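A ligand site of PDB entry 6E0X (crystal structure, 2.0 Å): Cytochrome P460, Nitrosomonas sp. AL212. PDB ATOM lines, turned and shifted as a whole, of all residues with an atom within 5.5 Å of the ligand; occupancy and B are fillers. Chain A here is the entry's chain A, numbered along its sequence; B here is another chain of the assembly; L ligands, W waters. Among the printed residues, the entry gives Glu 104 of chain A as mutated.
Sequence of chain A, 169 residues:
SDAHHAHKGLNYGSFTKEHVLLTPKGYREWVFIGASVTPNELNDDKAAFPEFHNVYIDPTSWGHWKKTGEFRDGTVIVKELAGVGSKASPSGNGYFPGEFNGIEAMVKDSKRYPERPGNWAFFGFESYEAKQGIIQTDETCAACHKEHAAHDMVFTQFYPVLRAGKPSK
Water W2 lies within hydrogen-bond range of O3 of the ligand (2.7 Å) and OH of Tyr 159 (3.0 Å). Water W1 lies within hydrogen-bond range of the backbone NH (N) of Cys 144 (2.6 Å), the backbone carbonyl oxygen (O) of Glu 139 (2.8 Å) and the backbone carbonyl oxygen (O) of Cys 141 (3.5 Å).
CE2 of Phe 49 touches N2 of the ligand, at 3.7 Å. CG1 of Val 55 touches C10 of the ligand, 3.9 Å away. Ile 77 touches the ligand. OE1 of Glu 104 touches C17 of the ligand (3.7 Å). Met 106 touches the ligand (SD to C9, 3.5 Å). Phe 122 touches the ligand. O of Phe 123 touches C17 of the ligand (3.5 Å). Thr 140 touches the ligand. Met 153 touches the ligand (O to O1, 3.7 Å). CA of Val 154 touches O1 of the ligand, at 3.4 Å. CD2 of Phe 158 touches C33 of the ligand (3.6 Å). OG of Ser 89 of chain B touches C31 of the ligand (3.3 Å). O of Pro 90 of chain B touches C26 of the ligand, at 3.4 Å. CE1 of Phe 96 of chain B touches O4 of the ligand, 3.5 Å away. Of the 30 residues printed, 22 come within 4 Å of the ligand. The nearest printed residue that does not touch the ligand is Ser 36 (4.01 Å).
The backbone NH of Phe 123 sits at hydrogen-bond distance from the backbone carbonyl oxygen of Ala 105. The backbone NH (N) of Met 106 sits at hydrogen-bond distance from the backbone carbonyl oxygen (O) of Ile 77, at 3.0 Å. The backbone NH (N) of Gln 136 is in hydrogen-bond range of the backbone carbonyl oxygen (O) of Phe 122 (3.0 Å). The backbone carbonyl oxygen (O) of Phe 49 lies within hydrogen-bond range of the side-chain hydroxyl (OG1) of Thr 38 (3.0 Å). The backbone carbonyl oxygen (O) of Met 153 sits at hydrogen-bond distance from a ring nitrogen (ND1) of His 145. O of Ser 36 lies within hydrogen-bond range of N of His 53 (2.9 Å). A ring nitrogen (NE2) of His 53 is in hydrogen-bond range of the backbone carbonyl oxygen (O) of Phe 49 (2.5 Å). A ring nitrogen (NE2) of His 53 lies within hydrogen-bond range of the side-chain hydroxyl (OG1) of Thr 38, 3.3 Å away.
NZ of Lys 79 is bonded to C1 of the ligand (1.4 Å). The side-chain hydroxyl (OG) of Ser 91 of chain B is in hydrogen-bond range of an oxygen (O4) of the ligand (2.5 Å). The side-chain sulfur (SG) of Cys 141 is bonded to a carbon (C18) of the ligand, 1.8 Å away. An oxygen (O3) of the ligand lies within hydrogen-bond range of a ring nitrogen (ND1) of His 53 (2.6 Å). The side-chain sulfur of Cys 144 is bonded to a carbon (C25) of the ligand (1.8 Å). OH of Tyr 159 sits at hydrogen-bond distance from O2 of the ligand (2.5 Å). An iron atom (FE1) of the ligand is bound by a ring nitrogen (NE2) of His 145, at 2.4 Å. An oxygen (O1) of the ligand sits at hydrogen-bond distance from the backbone NH of Phe 155 (3.1 Å).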
ATOM      1  N   SER A  36      32.214  28.740 -21.716  1.00  0.00           N
ATOM      2  CA  SER A  36      32.583  27.380 -21.356  1.00  0.00           C
ATOM      3  C   SER A  36      32.282  26.449 -22.522  1.00  0.00           C
ATOM      4  O   SER A  36      31.618  26.841 -23.488  1.00  0.00           O
ATOM      5  CB  SER A  36      31.831  26.917 -20.096  1.00  0.00           C
ATOM      6  OG  SER A  36      32.290  27.630 -18.974  1.00  0.00           O
ATOM      7  N   THR A  38      30.966  22.275 -23.258  1.00  0.00           N
ATOM      8  CA  THR A  38      30.610  20.909 -22.919  1.00  0.00           C
ATOM      9  C   THR A  38      30.487  20.153 -24.231  1.00  0.00           C
ATOM     10  O   THR A  38      29.423  20.173 -24.878  1.00  0.00           O
ATOM     11  CB  THR A  38      29.294  20.822 -22.123  1.00  0.00           C
ATOM     12  OG1 THR A  38      28.228  21.438 -22.852  1.00  0.00           O
ATOM     13  CG2 THR A  38      29.431  21.527 -20.778  1.00  0.00           C
ATOM     14  N   PHE A  49      23.716  20.992 -23.097  1.00  0.00           N
ATOM     15  CA  PHE A  49      23.746  22.258 -23.822  1.00  0.00           C
ATOM     16  C   PHE A  49      24.911  22.187 -24.813  1.00  0.00           C
ATOM     17  O   PHE A  49      26.034  22.636 -24.510  1.00  0.00           O
ATOM     18  CB  PHE A  49      23.925  23.464 -22.886  1.00  0.00           C
ATOM     19  CG  PHE A  49      22.649  23.920 -22.170  1.00  0.00           C
ATOM     20  CD1 PHE A  49      21.396  23.448 -22.539  1.00  0.00           C
ATOM     21  CD2 PHE A  49      22.737  24.854 -21.121  1.00  0.00           C
ATOM     22  CE1 PHE A  49      20.242  23.880 -21.855  1.00  0.00           C
ATOM     23  CE2 PHE A  49      21.595  25.289 -20.444  1.00  0.00           C
ATOM     24  CZ  PHE A  49      20.347  24.815 -20.820  1.00  0.00           C
ATOM     25  N   HIS A  53      29.204  27.589 -24.943  1.00  0.00           N
ATOM     26  CA  HIS A  53      28.225  28.533 -24.398  1.00  0.00           C
ATOM     27  C   HIS A  53      28.928  29.865 -24.223  1.00  0.00           C
ATOM     28  O   HIS A  53      29.906  29.944 -23.474  1.00  0.00           O
ATOM     29  CB  HIS A  53      27.633  28.075 -23.041  1.00  0.00           C
ATOM     30  CG  HIS A  53      27.398  26.590 -22.898  1.00  0.00           C
ATOM     31  ND1 HIS A  53      27.517  25.945 -21.688  1.00  0.00           N
ATOM     32  CD2 HIS A  53      27.058  25.645 -23.802  1.00  0.00           C
ATOM     33  CE1 HIS A  53      27.273  24.658 -21.845  1.00  0.00           C
ATOM     34  NE2 HIS A  53      26.992  24.446 -23.125  1.00  0.00           N
ATOM     35  N   VAL A  55      28.179  33.690 -22.860  1.00  0.00           N
ATOM     36  CA  VAL A  55      27.175  34.269 -21.957  1.00  0.00           C
ATOM     37  C   VAL A  55      27.288  35.782 -21.929  1.00  0.00           C
ATOM     38  O   VAL A  55      28.402  36.338 -21.950  1.00  0.00           O
ATOM     39  CB  VAL A  55      27.321  33.666 -20.544  1.00  0.00           C
ATOM     40  CG1 VAL A  55      26.143  34.122 -19.658  1.00  0.00           C
ATOM     41  CG2 VAL A  55      27.337  32.173 -20.646  1.00  0.00           C
ATOM     42  N   ILE A  77      20.091  37.812 -18.549  1.00  0.00           N
ATOM     43  CA  ILE A  77      21.288  37.080 -18.946  1.00  0.00           C
ATOM     44  C   ILE A  77      20.912  36.142 -20.070  1.00  0.00           C
ATOM     45  O   ILE A  77      19.905  35.433 -19.974  1.00  0.00           O
ATOM     46  CB  ILE A  77      21.888  36.315 -17.757  1.00  0.00           C
ATOM     47  CG1 ILE A  77      22.474  37.300 -16.739  1.00  0.00           C
ATOM     48  CG2 ILE A  77      22.943  35.245 -18.239  1.00  0.00           C
ATOM     49  CD1 ILE A  77      22.662  36.700 -15.339  1.00  0.00           C
ATOM     50  N   VAL A  78      21.720  36.121 -21.129  1.00  0.00           N
ATOM     51  CA  VAL A  78      21.491  35.290 -22.305  1.00  0.00           C
ATOM     52  C   VAL A  78      22.673  34.347 -22.493  1.00  0.00           C
ATOM     53  O   VAL A  78      23.836  34.783 -22.503  1.00  0.00           O
ATOM     54  CB  VAL A  78      21.254  36.155 -23.554  1.00  0.00           C
ATOM     55  CG1 VAL A  78      21.389  35.338 -24.827  1.00  0.00           C
ATOM     56  CG2 VAL A  78      19.871  36.840 -23.458  1.00  0.00           C
ATOM     57  N   LYS A  79      22.388  33.050 -22.623  1.00  0.00           N
ATOM     58  CA  LYS A  79      23.395  32.032 -22.899  1.00  0.00           C
ATOM     59  C   LYS A  79      23.216  31.558 -24.337  1.00  0.00           C
ATOM     60  O   LYS A  79      22.188  30.967 -24.668  1.00  0.00           O
ATOM     61  CB  LYS A  79      23.278  30.839 -21.936  1.00  0.00           C
ATOM     62  CG  LYS A  79      24.269  29.694 -22.258  1.00  0.00           C
ATOM     63  CD  LYS A  79      24.360  28.694 -21.078  1.00  0.00           C
ATOM     64  CE  LYS A  79      25.384  29.169 -20.066  1.00  0.00           C
ATOM     65  NZ  LYS A  79      25.323  28.415 -18.774  1.00  0.00           N
ATOM     66  N   GLU A 104      19.451  30.352 -24.459  1.00  0.00           N
ATOM     67  CA  GLU A 104      18.671  30.279 -23.232  1.00  0.00           C
ATOM     68  C   GLU A 104      18.801  31.613 -22.518  1.00  0.00           C
ATOM     69  O   GLU A 104      19.746  32.368 -22.764  1.00  0.00           O
ATOM     70  CB  GLU A 104      19.143  29.167 -22.294  1.00  0.00           C
ATOM     71  CG  GLU A 104      19.751  27.947 -22.970  1.00  0.00           C
ATOM     72  CD  GLU A 104      18.726  26.948 -23.454  1.00  0.00           C
ATOM     73  OE1 GLU A 104      17.585  26.940 -22.920  1.00  0.00           O
ATOM     74  OE2 GLU A 104      19.047  26.157 -24.374  1.00  0.00           O
ATOM     75  N   ALA A 105      17.862  31.892 -21.620  1.00  0.00           N
ATOM     76  CA  ALA A 105      17.843  33.194 -20.968  1.00  0.00           C
ATOM     77  C   ALA A 105      17.251  33.077 -19.581  1.00  0.00           C
ATOM     78  O   ALA A 105      16.426  32.195 -19.318  1.00  0.00           O
ATOM     79  CB  ALA A 105      17.059  34.236 -21.802  1.00  0.00           C
ATOM     80  N   MET A 106      17.648  33.993 -18.696  1.00  0.00           N
ATOM     81  CA  MET A 106      16.975  34.123 -17.404  1.00  0.00           C
ATOM     82  C   MET A 106      16.819  35.602 -17.094  1.00  0.00           C
ATOM     83  O   MET A 106      17.691  36.405 -17.428  1.00  0.00           O
ATOM     84  CB  MET A 106      17.752  33.443 -16.268  1.00  0.00           C
ATOM     85  CG  MET A 106      19.214  33.863 -16.157  1.00  0.00           C
ATOM     86  SD  MET A 106      20.211  32.579 -15.285  1.00  0.00           S
ATOM     87  CE  MET A 106      19.465  32.731 -13.676  1.00  0.00           C
ATOM     88  N   PHE A 122      13.134  31.464 -16.065  1.00  0.00           N
ATOM     89  CA  PHE A 122      14.001  30.778 -17.016  1.00  0.00           C
ATOM     90  C   PHE A 122      13.253  30.573 -18.331  1.00  0.00           C
ATOM     91  O   PHE A 122      12.114  30.088 -18.319  1.00  0.00           O
ATOM     92  CB  PHE A 122      14.476  29.442 -16.451  1.00  0.00           C
ATOM     93  CG  PHE A 122      15.546  29.564 -15.382  1.00  0.00           C
ATOM     94  CD1 PHE A 122      15.209  29.790 -14.058  1.00  0.00           C
ATOM     95  CD2 PHE A 122      16.898  29.462 -15.713  1.00  0.00           C
ATOM     96  CE1 PHE A 122      16.176  29.916 -13.081  1.00  0.00           C
ATOM     97  CE2 PHE A 122      17.875  29.578 -14.740  1.00  0.00           C
ATOM     98  CZ  PHE A 122      17.516  29.816 -13.419  1.00  0.00           C
ATOM     99  N   PHE A 123      13.868  30.916 -19.460  1.00  0.00           N
ATOM    100  CA  PHE A 123      13.206  30.811 -20.754  1.00  0.00           C
ATOM    101  C   PHE A 123      14.001  29.951 -21.712  1.00  0.00           C
ATOM    102  O   PHE A 123      15.212  30.133 -21.854  1.00  0.00           O
ATOM    103  CB  PHE A 123      12.976  32.200 -21.385  1.00  0.00           C
ATOM    104  CG  PHE A 123      12.049  33.068 -20.595  1.00  0.00           C
ATOM    105  CD1 PHE A 123      10.671  32.972 -20.765  1.00  0.00           C
ATOM    106  CD2 PHE A 123      12.544  33.954 -19.660  1.00  0.00           C
ATOM    107  CE1 PHE A 123       9.818  33.773 -20.034  1.00  0.00           C
ATOM    108  CE2 PHE A 123      11.690  34.770 -18.923  1.00  0.00           C
ATOM    109  CZ  PHE A 123      10.333  34.668 -19.103  1.00  0.00           C
ATOM    110  N   GLY A 124      13.302  29.043 -22.390  1.00  0.00           N
ATOM    111  CA  GLY A 124      13.826  28.371 -23.556  1.00  0.00           C
ATOM    112  C   GLY A 124      13.262  28.992 -24.830  1.00  0.00           C
ATOM    113  O   GLY A 124      12.211  29.622 -24.806  1.00  0.00           O
ATOM    114  N   GLN A 136       9.773  28.227 -18.007  1.00  0.00           N
ATOM    115  CA  GLN A 136      10.061  26.863 -17.596  1.00  0.00           C
ATOM    116  C   GLN A 136       9.662  26.607 -16.150  1.00  0.00           C
ATOM    117  O   GLN A 136       9.751  27.494 -15.298  1.00  0.00           O
ATOM    118  CB  GLN A 136      11.562  26.556 -17.782  1.00  0.00           C
ATOM    119  CG  GLN A 136      12.068  26.883 -19.165  1.00  0.00           C
ATOM    120  CD  GLN A 136      11.616  25.860 -20.181  1.00  0.00           C
ATOM    121  OE1 GLN A 136      11.610  24.662 -19.903  1.00  0.00           O
ATOM    122  NE2 GLN A 136      11.211  26.319 -21.361  1.00  0.00           N
ATOM    123  N   GLU A 139      11.575  22.952 -11.602  1.00  0.00           N
ATOM    124  CA  GLU A 139      12.428  21.774 -11.642  1.00  0.00           C
ATOM    125  C   GLU A 139      13.292  21.731 -12.886  1.00  0.00           C
ATOM    126  O   GLU A 139      14.372  21.135 -12.879  1.00  0.00           O
ATOM    127  CB  GLU A 139      11.573  20.503 -11.554  1.00  0.00           C
ATOM    128  CG  GLU A 139      10.580  20.384 -12.698  1.00  0.00           C
ATOM    129  CD  GLU A 139       9.859  19.051 -12.743  1.00  0.00           C
ATOM    130  OE1 GLU A 139       9.959  18.263 -11.764  1.00  0.00           O
ATOM    131  OE2 GLU A 139       9.188  18.786 -13.768  1.00  0.00           O
ATOM    132  N   THR A 140      12.838  22.350 -13.982  1.00  0.00           N
ATOM    133  CA  THR A 140      13.525  22.175 -15.255  1.00  0.00           C
ATOM    134  C   THR A 140      14.811  22.981 -15.351  1.00  0.00           C
ATOM    135  O   THR A 140      15.718  22.612 -16.104  1.00  0.00           O
ATOM    136  CB  THR A 140      12.588  22.561 -16.404  1.00  0.00           C
ATOM    137  OG1 THR A 140      11.311  21.934 -16.208  1.00  0.00           O
ATOM    138  CG2 THR A 140      13.147  22.134 -17.765  1.00  0.00           C
ATOM    139  N   CYS A 141      14.918  24.072 -14.588  1.00  0.00           N
ATOM    140  CA  CYS A 141      16.064  24.950 -14.709  1.00  0.00           C
ATOM    141  C   CYS A 141      16.510  25.471 -13.347  1.00  0.00           C
ATOM    142  O   CYS A 141      17.665  25.308 -12.976  1.00  0.00           O
ATOM    143  CB  CYS A 141      15.737  26.140 -15.634  1.00  0.00           C
ATOM    144  SG  CYS A 141      14.925  25.695 -17.169  1.00  0.00           S
ATOM    145  N   CYS A 144      18.583  23.025 -10.479  1.00  0.00           N
ATOM    146  CA  CYS A 144      20.034  22.890 -10.607  1.00  0.00           C
ATOM    147  C   CYS A 144      20.754  24.208 -10.338  1.00  0.00           C
ATOM    148  O   CYS A 144      21.813  24.218  -9.702  1.00  0.00           O
ATOM    149  CB  CYS A 144      20.399  22.351 -11.988  1.00  0.00           C
ATOM    150  SG  CYS A 144      22.176  22.237 -12.341  1.00  0.00           S
ATOM    151  N   HIS A 145      20.184  25.337 -10.808  1.00  0.00           N
ATOM    152  CA  HIS A 145      20.834  26.623 -10.569  1.00  0.00           C
ATOM    153  C   HIS A 145      20.867  26.992  -9.078  1.00  0.00           C
ATOM    154  O   HIS A 145      21.871  27.522  -8.581  1.00  0.00           O
ATOM    155  CB  HIS A 145      20.148  27.719 -11.386  1.00  0.00           C
ATOM    156  CG  HIS A 145      20.708  27.879 -12.779  1.00  0.00           C
ATOM    157  ND1 HIS A 145      21.389  29.009 -13.183  1.00  0.00           N
ATOM    158  CD2 HIS A 145      20.686  27.058 -13.856  1.00  0.00           C
ATOM    159  CE1 HIS A 145      21.753  28.873 -14.445  1.00  0.00           C
ATOM    160  NE2 HIS A 145      21.334  27.699 -14.879  1.00  0.00           N
ATOM    161  N   ALA A 149      24.881  27.148  -8.157  1.00  0.00           N
ATOM    162  CA  ALA A 149      25.476  28.404  -8.594  1.00  0.00           C
ATOM    163  C   ALA A 149      26.114  29.149  -7.417  1.00  0.00           C
ATOM    164  O   ALA A 149      25.589  29.141  -6.312  1.00  0.00           O
ATOM    165  CB  ALA A 149      24.426  29.293  -9.266  1.00  0.00           C
ATOM    166  N   MET A 153      21.832  32.315  -7.869  1.00  0.00           N
ATOM    167  CA  MET A 153      21.442  31.357  -8.903  1.00  0.00           C
ATOM    168  C   MET A 153      22.155  31.563 -10.235  1.00  0.00           C
ATOM    169  O   MET A 153      21.816  30.905 -11.223  1.00  0.00           O
ATOM    170  CB  MET A 153      19.915  31.349  -9.106  1.00  0.00           C
ATOM    171  CG  MET A 153      19.154  30.741  -7.909  1.00  0.00           C
ATOM    172  SD  MET A 153      17.391  31.085  -7.958  1.00  0.00           S
ATOM    173  CE  MET A 153      16.826  30.031  -9.296  1.00  0.00           C
ATOM    174  N   VAL A 154      23.169  32.414 -10.292  1.00  0.00           N
ATOM    175  CA  VAL A 154      23.995  32.568 -11.491  1.00  0.00           C
ATOM    176  C   VAL A 154      25.356  31.929 -11.214  1.00  0.00           C
ATOM    177  O   VAL A 154      25.973  32.187 -10.170  1.00  0.00           O
ATOM    178  CB  VAL A 154      24.157  34.043 -11.894  1.00  0.00           C
ATOM    179  CG1 VAL A 154      25.138  34.188 -13.064  1.00  0.00           C
ATOM    180  CG2 VAL A 154      22.811  34.658 -12.274  1.00  0.00           C
ATOM    181  N   PHE A 155      25.835  31.113 -12.158  1.00  0.00           N
ATOM    182  CA  PHE A 155      27.086  30.376 -11.986  1.00  0.00           C
ATOM    183  C   PHE A 155      28.325  31.259 -12.080  1.00  0.00           C
ATOM    184  O   PHE A 155      29.197  31.030 -12.935  1.00  0.00           O
ATOM    185  CB  PHE A 155      27.168  29.246 -13.009  1.00  0.00           C
ATOM    186  CG  PHE A 155      26.325  28.046 -12.629  1.00  0.00           C
ATOM    187  CD1 PHE A 155      26.812  27.093 -11.746  1.00  0.00           C
ATOM    188  CD2 PHE A 155      25.039  27.885 -13.141  1.00  0.00           C
ATOM    189  CE1 PHE A 155      26.040  25.993 -11.376  1.00  0.00           C
ATOM    190  CE2 PHE A 155      24.263  26.778 -12.782  1.00  0.00           C
ATOM    191  CZ  PHE A 155      24.775  25.826 -11.898  1.00  0.00           C
ATOM    192  N   PHE A 158      32.046  30.584 -13.129  1.00  0.00           N
ATOM    193  CA  PHE A 158      32.483  30.474 -14.509  1.00  0.00           C
ATOM    194  C   PHE A 158      32.401  31.788 -15.285  1.00  0.00           C
ATOM    195  O   PHE A 158      32.484  31.763 -16.518  1.00  0.00           O
ATOM    196  CB  PHE A 158      31.677  29.381 -15.222  1.00  0.00           C
ATOM    197  CG  PHE A 158      31.640  28.076 -14.467  1.00  0.00           C
ATOM    198  CD1 PHE A 158      32.815  27.471 -14.032  1.00  0.00           C
ATOM    199  CD2 PHE A 158      30.427  27.443 -14.211  1.00  0.00           C
ATOM    200  CE1 PHE A 158      32.779  26.245 -13.343  1.00  0.00           C
ATOM    201  CE2 PHE A 158      30.394  26.231 -13.524  1.00  0.00           C
ATOM    202  CZ  PHE A 158      31.567  25.641 -13.082  1.00  0.00           C
ATOM    203  N   TYR A 159      32.245  32.929 -14.597  1.00  0.00           N
ATOM    204  CA  TYR A 159      32.145  34.242 -15.242  1.00  0.00           C
ATOM    205  C   TYR A 159      33.254  35.110 -14.668  1.00  0.00           C
ATOM    206  O   TYR A 159      33.034  35.928 -13.758  1.00  0.00           O
ATOM    207  CB  TYR A 159      30.755  34.878 -15.091  1.00  0.00           C
ATOM    208  CG  TYR A 159      29.737  33.945 -15.669  1.00  0.00           C
ATOM    209  CD1 TYR A 159      29.937  33.399 -16.939  1.00  0.00           C
ATOM    210  CD2 TYR A 159      28.628  33.524 -14.943  1.00  0.00           C
ATOM    211  CE1 TYR A 159      29.051  32.485 -17.484  1.00  0.00           C
ATOM    212  CE2 TYR A 159      27.747  32.596 -15.470  1.00  0.00           C
ATOM    213  CZ  TYR A 159      27.968  32.089 -16.739  1.00  0.00           C
ATOM    214  OH  TYR A 159      27.104  31.163 -17.281  1.00  0.00           O
ATOM    215  N   SER B  89      31.217  20.051 -14.366  1.00  0.00           N
ATOM    216  CA  SER B  89      30.281  20.961 -13.719  1.00  0.00           C
ATOM    217  C   SER B  89      28.917  20.301 -13.762  1.00  0.00           C
ATOM    218  O   SER B  89      28.781  19.285 -14.455  1.00  0.00           O
ATOM    219  CB  SER B  89      30.246  22.324 -14.435  1.00  0.00           C
ATOM    220  OG  SER B  89      29.121  22.366 -15.296  1.00  0.00           O
ATOM    221  N   PRO B  90      27.886  20.861 -13.114  1.00  0.00           N
ATOM    222  CA  PRO B  90      26.544  20.279 -13.246  1.00  0.00           C
ATOM    223  C   PRO B  90      26.010  20.232 -14.660  1.00  0.00           C
ATOM    224  O   PRO B  90      25.066  19.469 -14.925  1.00  0.00           O
ATOM    225  CB  PRO B  90      25.683  21.189 -12.360  1.00  0.00           C
ATOM    226  CG  PRO B  90      26.619  21.665 -11.325  1.00  0.00           C
ATOM    227  CD  PRO B  90      27.939  21.864 -12.043  1.00  0.00           C
ATOM    228  N   SER B  91      26.562  21.033 -15.577  1.00  0.00           N
ATOM    229  CA  SER B  91      26.127  20.967 -16.967  1.00  0.00           C
ATOM    230  C   SER B  91      26.819  19.859 -17.756  1.00  0.00           C
ATOM    231  O   SER B  91      26.430  19.630 -18.915  1.00  0.00           O
ATOM    232  CB  SER B  91      26.354  22.323 -17.666  1.00  0.00           C
ATOM    233  OG  SER B  91      27.744  22.563 -17.888  1.00  0.00           O
ATOM    234  N   PHE B  96      35.958  24.643 -18.331  1.00  0.00           N
ATOM    235  CA  PHE B  96      35.286  25.768 -17.712  1.00  0.00           C
ATOM    236  C   PHE B  96      36.355  26.722 -17.217  1.00  0.00           C
ATOM    237  O   PHE B  96      37.368  26.271 -16.664  1.00  0.00           O
ATOM    238  CB  PHE B  96      34.412  25.299 -16.541  1.00  0.00           C
ATOM    239  CG  PHE B  96      33.396  24.275 -16.920  1.00  0.00           C
ATOM    240  CD1 PHE B  96      32.131  24.669 -17.339  1.00  0.00           C
ATOM    241  CD2 PHE B  96      33.714  22.933 -16.907  1.00  0.00           C
ATOM    242  CE1 PHE B  96      31.193  23.745 -17.712  1.00  0.00           C
ATOM    243  CE2 PHE B  96      32.785  21.999 -17.284  1.00  0.00           C
ATOM    244  CZ  PHE B  96      31.514  22.411 -17.688  1.00  0.00           C
HETATM  245 FE1  LIG L   1      21.569  26.473 -16.880  1.00  0.00          FE
HETATM  246  C1  LIG L   1      24.464  28.251 -17.649  1.00  0.00           C
HETATM  247  C2  LIG L   1      19.752  28.734 -18.637  1.00  0.00           C
HETATM  248  C3  LIG L   1      18.871  24.350 -16.733  1.00  0.00           C
HETATM  249  C4  LIG L   1      23.428  24.243 -15.085  1.00  0.00           C
HETATM  250  N1  LIG L   1      22.064  28.157 -18.135  1.00  0.00           N
HETATM  251  C5  LIG L   1      23.242  28.845 -17.921  1.00  0.00           C
HETATM  252  C6  LIG L   1      22.978  30.261 -18.063  1.00  0.00           C
HETATM  253  C7  LIG L   1      21.676  30.397 -18.332  1.00  0.00           C
HETATM  254  C8  LIG L   1      21.070  29.068 -18.374  1.00  0.00           C
HETATM  255  C9  LIG L   1      20.952  31.749 -18.594  1.00  0.00           C
HETATM  256  C10 LIG L   1      24.003  31.407 -17.909  1.00  0.00           C
HETATM  257  C11 LIG L   1      23.889  31.993 -16.520  1.00  0.00           C
HETATM  258  C12 LIG L   1      24.396  30.989 -15.473  1.00  0.00           C
HETATM  259  O1  LIG L   1      23.732  30.867 -14.428  1.00  0.00           O
HETATM  260  O2  LIG L   1      25.432  30.316 -15.693  1.00  0.00           O
HETATM  261  N2  LIG L   1      19.647  26.524 -17.549  1.00  0.00           N
HETATM  262  C13 LIG L   1      19.094  27.553 -18.301  1.00  0.00           C
HETATM  263  C14 LIG L   1      17.741  27.157 -18.661  1.00  0.00           C
HETATM  264  C15 LIG L   1      17.501  25.957 -18.126  1.00  0.00           C
HETATM  265  C16 LIG L   1      18.698  25.527 -17.430  1.00  0.00           C
HETATM  266  C17 LIG L   1      16.720  28.016 -19.462  1.00  0.00           C
HETATM  267  C18 LIG L   1      16.194  25.142 -18.249  1.00  0.00           C
HETATM  268  C19 LIG L   1      15.956  24.763 -19.732  1.00  0.00           C
HETATM  269  N3  LIG L   1      21.228  24.623 -16.071  1.00  0.00           N
HETATM  270  C20 LIG L   1      20.028  23.949 -16.102  1.00  0.00           C
HETATM  271  C21 LIG L   1      20.209  22.682 -15.412  1.00  0.00           C
HETATM  272  C22 LIG L   1      21.443  22.667 -14.884  1.00  0.00           C
HETATM  273  C23 LIG L   1      22.119  23.888 -15.326  1.00  0.00           C
HETATM  274  C24 LIG L   1      18.997  21.743 -15.195  1.00  0.00           C
HETATM  275  C25 LIG L   1      22.080  21.558 -13.973  1.00  0.00           C
HETATM  276  C26 LIG L   1      21.765  20.175 -14.542  1.00  0.00           C
HETATM  277  N4  LIG L   1      23.657  26.296 -16.439  1.00  0.00           N
HETATM  278  C27 LIG L   1      24.172  25.255 -15.670  1.00  0.00           C
HETATM  279  C28 LIG L   1      25.614  25.411 -15.550  1.00  0.00           C
HETATM  280  C29 LIG L   1      25.968  26.666 -16.352  1.00  0.00           C
HETATM  281  C30 LIG L   1      24.685  27.141 -16.861  1.00  0.00           C
HETATM  282  C31 LIG L   1      26.610  24.510 -14.775  1.00  0.00           C
HETATM  283  C32 LIG L   1      27.374  27.309 -16.540  1.00  0.00           C
HETATM  284  C33 LIG L   1      28.472  26.362 -17.076  1.00  0.00           C
HETATM  285  C34 LIG L   1      28.131  26.051 -18.492  1.00  0.00           C
HETATM  286  O3  LIG L   1      27.896  26.992 -19.316  1.00  0.00           O
HETATM  287  O4  LIG L   1      28.097  24.844 -18.789  1.00  0.00           O
HETATM  288  O   HOH W   1      17.030  21.962 -12.322  1.00  0.00           O
HETATM  289  O   HOH W   2      28.956  29.451 -18.951  1.00  0.00           O
